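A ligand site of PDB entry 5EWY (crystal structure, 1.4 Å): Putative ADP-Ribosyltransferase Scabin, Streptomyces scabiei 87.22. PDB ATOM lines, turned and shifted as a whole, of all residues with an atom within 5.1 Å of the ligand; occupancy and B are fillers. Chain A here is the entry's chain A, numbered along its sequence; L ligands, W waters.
The backbone NH (N) of Ser 78 sits at hydrogen-bond distance from an oxygen (O1) of the ligand. A nitrogen (N2) of the ligand sits at hydrogen-bond distance from the backbone carbonyl oxygen (O) of Ser 78. An oxygen (O3) of the ligand lies within salt-bridge range of the guanidinium group of Arg 77. NZ of Lys 94 is in salt-bridge range of O2 of the ligand, at 3.6 Å.
The guanidinium group (NH2) of Arg 77 sits at hydrogen-bond distance from the backbone carbonyl oxygen (O) of Ser 117. The side-chain carboxylate (OD2) of Asp 79 lies within salt-bridge range of the guanidinium group (NE) of Arg 77 (2.9 Å). The side-chain carboxylate (OE2) of Glu 160 lies within hydrogen-bond range of the side-chain hydroxyl (OG) of Ser 117. The backbone NH of Val 161 lies within hydrogen-bond range of the backbone carbonyl oxygen of Thr 118. The backbone carbonyl oxygen (O) of Gln 158 lies within hydrogen-bond range of the side-chain hydroxyl (OG1) of Thr 119, 2.7 Å away. OH of Tyr 106 sits at hydrogen-bond distance from OG of Ser 117 (2.5 Å). The backbone NH (N) of Thr 119 lies within hydrogen-bond range of the backbone carbonyl oxygen (O) of Tyr 76 (2.8 Å). The side-chain hydroxyl (OG1) of Thr 119 lies within hydrogen-bond range of the backbone carbonyl oxygen (O) of Val 159 (3.4 Å).
The backbone carbonyl oxygen (O) of Thr 118 sits close to a fluorine (F1) of the ligand, at 3.3 Å. The backbone carbonyl oxygen (O) of Gln 158 sits close to a fluorine (F1) of the ligand, 3.4 Å away. Merely in contact with the ligand: Glu 160, Trp 128, Ser 117, Leu 124, Thr 119 and Asn 110. Hydrophobic or aromatic side chains within 4 Å of the ligand: Leu 124 and Trp 128. 11 residues have an atom within 4 Å of the ligand: Arg 77, Ser 78, Lys 94, Asn 110, Ser 117, Thr 118, Thr 119, Leu 124, Trp 128, Gln 158 and Glu 160. Along chain A the residues within 4 Å of the ligand span positions 77 to 160. The nearest printed residue that does not touch the ligand is Tyr 76 (4.2 Å).
Water W5 lies within hydrogen-bond range of O2 of the ligand (2.8 Å) and NH1 of Arg 77 (3.5 Å). Water W3 bridges an oxygen (O1) of the ligand (2.9 Å) and the backbone NH (N) of Ser 78 (3.4 Å). Water W1 lies within hydrogen-bond range of OH of Tyr 106 (2.8 Å), N of Ser 117 (2.9 Å), NH2 of Arg 77 (3.0 Å) and O3 of the ligand (3.2 Å). Water W4 lies within hydrogen-bond range of OH of Tyr 106 and OG of Ser 117.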
ATOM      1  N   TYR A  76      -3.007  18.176  28.881  1.00  0.00           N
ATOM      2  CA  TYR A  76      -2.381  18.483  30.156  1.00  0.00           C
ATOM      3  C   TYR A  76      -1.120  19.304  29.933  1.00  0.00           C
ATOM      4  O   TYR A  76      -0.493  19.232  28.883  1.00  0.00           O
ATOM      5  CB  TYR A  76      -2.036  17.201  30.967  1.00  0.00           C
ATOM      6  CG  TYR A  76      -3.215  16.278  30.986  1.00  0.00           C
ATOM      7  CD1 TYR A  76      -3.423  15.362  29.966  1.00  0.00           C
ATOM      8  CD2 TYR A  76      -4.157  16.361  31.992  1.00  0.00           C
ATOM      9  CE1 TYR A  76      -4.554  14.562  29.937  1.00  0.00           C
ATOM     10  CE2 TYR A  76      -5.296  15.546  31.981  1.00  0.00           C
ATOM     11  CZ  TYR A  76      -5.423  14.656  30.970  1.00  0.00           C
ATOM     12  OH  TYR A  76      -6.567  13.882  30.945  1.00  0.00           O
ATOM     13  N   ARG A  77      -0.792  20.114  30.923  1.00  0.00           N
ATOM     14  CA  ARG A  77       0.462  20.844  30.912  1.00  0.00           C
ATOM     15  C   ARG A  77       1.003  20.913  32.333  1.00  0.00           C
ATOM     16  O   ARG A  77       0.329  21.453  33.224  1.00  0.00           O
ATOM     17  CB  ARG A  77       0.277  22.258  30.351  1.00  0.00           C
ATOM     18  CG  ARG A  77       1.573  23.062  30.430  1.00  0.00           C
ATOM     19  CD  ARG A  77       1.467  24.418  29.747  1.00  0.00           C
ATOM     20  NE  ARG A  77       2.608  25.255  30.122  1.00  0.00           N
ATOM     21  CZ  ARG A  77       3.812  25.221  29.572  1.00  0.00           C
ATOM     22  NH1 ARG A  77       4.766  26.009  30.041  1.00  0.00           N
ATOM     23  NH2 ARG A  77       4.068  24.454  28.521  1.00  0.00           N
ATOM     24  N   SER A  78       2.223  20.398  32.528  1.00  0.00           N
ATOM     25  CA  SER A  78       2.981  20.583  33.762  1.00  0.00           C
ATOM     26  C   SER A  78       3.594  21.986  33.703  1.00  0.00           C
ATOM     27  O   SER A  78       4.188  22.352  32.699  1.00  0.00           O
ATOM     28  CB  SER A  78       4.080  19.511  33.801  1.00  0.00           C
ATOM     29  OG  SER A  78       4.874  19.689  34.941  1.00  0.00           O
ATOM     30  N   ASP A  79       3.371  22.789  34.742  1.00  0.00           N
ATOM     31  CA  ASP A  79       3.934  24.140  34.761  1.00  0.00           C
ATOM     32  C   ASP A  79       4.197  24.504  36.216  1.00  0.00           C
ATOM     33  O   ASP A  79       3.377  24.249  37.091  1.00  0.00           O
ATOM     34  CB  ASP A  79       2.954  25.115  34.088  1.00  0.00           C
ATOM     35  CG  ASP A  79       3.613  26.362  33.556  1.00  0.00           C
ATOM     36  OD1 ASP A  79       4.511  26.909  34.242  1.00  0.00           O
ATOM     37  OD2 ASP A  79       3.234  26.804  32.441  1.00  0.00           O
ATOM     38  N   LYS A  94       6.260  32.327  24.905  1.00  0.00           N
ATOM     39  CA  LYS A  94       7.415  33.155  25.253  1.00  0.00           C
ATOM     40  C   LYS A  94       7.730  34.202  24.176  1.00  0.00           C
ATOM     41  O   LYS A  94       8.002  35.365  24.513  1.00  0.00           O
ATOM     42  CB  LYS A  94       8.623  32.257  25.572  1.00  0.00           C
ATOM     43  CG  LYS A  94       8.495  31.627  26.950  1.00  0.00           C
ATOM     44  CD  LYS A  94       9.687  30.782  27.340  1.00  0.00           C
ATOM     45  CE  LYS A  94       9.527  30.314  28.777  1.00  0.00           C
ATOM     46  NZ  LYS A  94      10.691  29.553  29.301  1.00  0.00           N
ATOM     47  N   TYR A 106      12.361  23.326  18.425  1.00  0.00           N
ATOM     48  CA  TYR A 106      11.806  23.695  19.727  1.00  0.00           C
ATOM     49  C   TYR A 106      11.737  22.499  20.658  1.00  0.00           C
ATOM     50  O   TYR A 106      12.072  22.598  21.848  1.00  0.00           O
ATOM     51  CB  TYR A 106      10.402  24.278  19.517  1.00  0.00           C
ATOM     52  CG  TYR A 106       9.529  24.359  20.753  1.00  0.00           C
ATOM     53  CD1 TYR A 106       9.823  25.262  21.760  1.00  0.00           C
ATOM     54  CD2 TYR A 106       8.416  23.544  20.898  1.00  0.00           C
ATOM     55  CE1 TYR A 106       9.039  25.338  22.891  1.00  0.00           C
ATOM     56  CE2 TYR A 106       7.625  23.613  22.032  1.00  0.00           C
ATOM     57  CZ  TYR A 106       7.942  24.520  23.031  1.00  0.00           C
ATOM     58  OH  TYR A 106       7.182  24.618  24.169  1.00  0.00           O
ATOM     59  N   ASN A 110      15.460  23.439  24.017  1.00  0.00           N
ATOM     60  CA  ASN A 110      14.608  24.413  24.666  1.00  0.00           C
ATOM     61  C   ASN A 110      15.044  25.821  24.255  1.00  0.00           C
ATOM     62  O   ASN A 110      16.219  26.185  24.400  1.00  0.00           O
ATOM     63  CB  ASN A 110      14.676  24.253  26.190  1.00  0.00           C
ATOM     64  CG  ASN A 110      13.659  25.100  26.926  1.00  0.00           C
ATOM     65  OD1 ASN A 110      12.699  25.607  26.332  1.00  0.00           O
ATOM     66  ND2 ASN A 110      13.857  25.265  28.228  1.00  0.00           N
ATOM     67  N   SER A 117       3.512  24.228  25.021  1.00  0.00           N
ATOM     68  CA  SER A 117       3.503  22.773  24.962  1.00  0.00           C
ATOM     69  C   SER A 117       2.471  22.207  25.916  1.00  0.00           C
ATOM     70  O   SER A 117       2.349  22.643  27.057  1.00  0.00           O
ATOM     71  CB  SER A 117       4.848  22.213  25.369  1.00  0.00           C
ATOM     72  OG  SER A 117       5.838  22.583  24.427  1.00  0.00           O
ATOM     73  N   THR A 118       1.748  21.203  25.435  1.00  0.00           N
ATOM     74  CA  THR A 118       0.813  20.408  26.220  1.00  0.00           C
ATOM     75  C   THR A 118       1.043  18.967  25.813  1.00  0.00           C
ATOM     76  O   THR A 118       1.773  18.668  24.875  1.00  0.00           O
ATOM     77  CB  THR A 118      -0.649  20.800  25.953  1.00  0.00           C
ATOM     78  OG1 THR A 118      -1.042  20.366  24.648  1.00  0.00           O
ATOM     79  CG2 THR A 118      -0.850  22.338  26.103  1.00  0.00           C
ATOM     80  N   THR A 119       0.352  18.055  26.504  1.00  0.00           N
ATOM     81  CA  THR A 119       0.489  16.640  26.209  1.00  0.00           C
ATOM     82  C   THR A 119      -0.859  15.939  26.257  1.00  0.00           C
ATOM     83  O   THR A 119      -1.732  16.288  27.032  1.00  0.00           O
ATOM     84  CB  THR A 119       1.489  15.974  27.196  1.00  0.00           C
ATOM     85  OG1 THR A 119       1.569  14.571  26.949  1.00  0.00           O
ATOM     86  CG2 THR A 119       1.099  16.205  28.625  1.00  0.00           C
ATOM     87  N   LEU A 124       2.339  12.841  32.370  1.00  0.00           N
ATOM     88  CA  LEU A 124       3.660  13.320  32.000  1.00  0.00           C
ATOM     89  C   LEU A 124       4.239  14.212  33.091  1.00  0.00           C
ATOM     90  O   LEU A 124       5.457  14.368  33.195  1.00  0.00           O
ATOM     91  CB  LEU A 124       3.592  14.061  30.663  1.00  0.00           C
ATOM     92  CG  LEU A 124       4.990  14.345  30.049  1.00  0.00           C
ATOM     93  CD1 LEU A 124       5.588  13.061  29.574  1.00  0.00           C
ATOM     94  CD2 LEU A 124       4.836  15.281  28.893  1.00  0.00           C
ATOM     95  N   TRP A 128       8.450  15.731  35.036  1.00  0.00           N
ATOM     96  CA  TRP A 128       8.882  17.114  35.127  1.00  0.00           C
ATOM     97  C   TRP A 128       9.152  17.421  36.596  1.00  0.00           C
ATOM     98  O   TRP A 128       8.227  17.638  37.376  1.00  0.00           O
ATOM     99  CB  TRP A 128       7.811  18.046  34.575  1.00  0.00           C
ATOM    100  CG  TRP A 128       7.670  17.980  33.095  1.00  0.00           C
ATOM    101  CD1 TRP A 128       6.675  17.387  32.382  1.00  0.00           C
ATOM    102  CD2 TRP A 128       8.577  18.518  32.132  1.00  0.00           C
ATOM    103  NE1 TRP A 128       6.903  17.529  31.036  1.00  0.00           N
ATOM    104  CE2 TRP A 128       8.058  18.224  30.858  1.00  0.00           C
ATOM    105  CE3 TRP A 128       9.766  19.232  32.233  1.00  0.00           C
ATOM    106  CZ2 TRP A 128       8.709  18.624  29.692  1.00  0.00           C
ATOM    107  CZ3 TRP A 128      10.404  19.618  31.072  1.00  0.00           C
ATOM    108  CH2 TRP A 128       9.864  19.325  29.827  1.00  0.00           C
ATOM    109  N   GLN A 158       6.667  12.063  24.877  1.00  0.00           N
ATOM    110  CA  GLN A 158       5.931  13.147  25.506  1.00  0.00           C
ATOM    111  C   GLN A 158       4.567  13.371  24.875  1.00  0.00           C
ATOM    112  O   GLN A 158       3.770  14.147  25.420  1.00  0.00           O
ATOM    113  CB  GLN A 158       6.696  14.450  25.399  1.00  0.00           C
ATOM    114  CG  GLN A 158       8.032  14.495  26.086  1.00  0.00           C
ATOM    115  CD  GLN A 158       8.581  15.909  26.049  1.00  0.00           C
ATOM    116  OE1 GLN A 158       8.732  16.528  24.955  1.00  0.00           O
ATOM    117  NE2 GLN A 158       8.866  16.452  27.216  1.00  0.00           N
ATOM    118  N   VAL A 159       4.304  12.767  23.717  1.00  0.00           N
ATOM    119  CA  VAL A 159       3.022  12.861  23.009  1.00  0.00           C
ATOM    120  C   VAL A 159       2.460  14.290  23.088  1.00  0.00           C
ATOM    121  O   VAL A 159       1.342  14.541  23.566  1.00  0.00           O
ATOM    122  CB  VAL A 159       2.030  11.753  23.410  1.00  0.00           C
ATOM    123  CG1 VAL A 159       2.558  10.396  22.983  1.00  0.00           C
ATOM    124  CG2 VAL A 159       1.717  11.766  24.901  1.00  0.00           C
ATOM    125  N   GLU A 160       3.234  15.217  22.547  1.00  0.00           N
ATOM    126  CA  GLU A 160       3.049  16.645  22.709  1.00  0.00           C
ATOM    127  C   GLU A 160       2.053  17.190  21.701  1.00  0.00           C
ATOM    128  O   GLU A 160       1.997  16.746  20.545  1.00  0.00           O
ATOM    129  CB  GLU A 160       4.395  17.356  22.556  1.00  0.00           C
ATOM    130  CG  GLU A 160       4.320  18.831  22.785  1.00  0.00           C
ATOM    131  CD  GLU A 160       5.643  19.524  22.685  1.00  0.00           C
ATOM    132  OE1 GLU A 160       6.675  18.830  22.663  1.00  0.00           O
ATOM    133  OE2 GLU A 160       5.627  20.773  22.646  1.00  0.00           O
ATOM    134  N   VAL A 161       1.307  18.190  22.135  1.00  0.00           N
ATOM    135  CA  VAL A 161       0.488  19.043  21.284  1.00  0.00           C
ATOM    136  C   VAL A 161       0.962  20.474  21.554  1.00  0.00           C
ATOM    137  O   VAL A 161       0.927  20.955  22.695  1.00  0.00           O
ATOM    138  CB  VAL A 161      -1.016  18.874  21.573  1.00  0.00           C
ATOM    139  CG1 VAL A 161      -1.846  19.835  20.724  1.00  0.00           C
ATOM    140  CG2 VAL A 161      -1.466  17.422  21.347  1.00  0.00           C
HETATM  141  N1  LIG L   1       8.636  23.052  29.410  1.00  0.00           N
HETATM  142  C1  LIG L   1       8.041  23.368  30.562  1.00  0.00           C
HETATM  143  C2  LIG L   1       9.935  23.704  29.036  1.00  0.00           C
HETATM  144  C3  LIG L   1       9.593  26.177  28.570  1.00  0.00           C
HETATM  145  C4  LIG L   1       4.580  18.765  27.702  1.00  0.00           C
HETATM  146  C5  LIG L   1       5.189  18.359  26.525  1.00  0.00           C
HETATM  147  C6  LIG L   1       6.379  18.940  26.100  1.00  0.00           C
HETATM  148  C7  LIG L   1       6.955  19.949  26.860  1.00  0.00           C
HETATM  149  C8  LIG L   1       6.373  20.358  28.081  1.00  0.00           C
HETATM  150  C9  LIG L   1       5.168  19.769  28.482  1.00  0.00           C
HETATM  151  C10 LIG L   1       4.556  20.177  29.742  1.00  0.00           C
HETATM  152  C11 LIG L   1       6.954  21.408  28.891  1.00  0.00           C
HETATM  153  C12 LIG L   1       6.280  21.742  30.092  1.00  0.00           C
HETATM  154  N2  LIG L   1       5.122  21.157  30.469  1.00  0.00           N
HETATM  155  C13 LIG L   1       8.150  22.085  28.603  1.00  0.00           C
HETATM  156  C14 LIG L   1       6.865  22.792  30.916  1.00  0.00           C
HETATM  157  C15 LIG L   1      10.139  25.132  29.516  1.00  0.00           C
HETATM  158  C16 LIG L   1       8.120  26.449  28.838  1.00  0.00           C
HETATM  159  O1  LIG L   1       3.477  19.647  30.122  1.00  0.00           O
HETATM  160  F1  LIG L   1       4.619  17.397  25.798  1.00  0.00           F
HETATM  161  O2  LIG L   1       7.718  27.632  28.877  1.00  0.00           O
HETATM  162  O3  LIG L   1       7.353  25.495  29.019  1.00  0.00           O
HETATM  163  O   HOH W   1       5.752  25.635  26.292  1.00  0.00           O
HETATM  164  O   HOH W   2       6.520  29.119  30.829  1.00  0.00           O
HETATM  165  O   HOH W   3       3.305  17.248  31.660  1.00  0.00           O
HETATM  166  O   HOH W   4       8.882  22.529  25.471  1.00  0.00           O
HETATM  167  O   HOH W   5       5.431  28.201  27.434  1.00  0.00           O
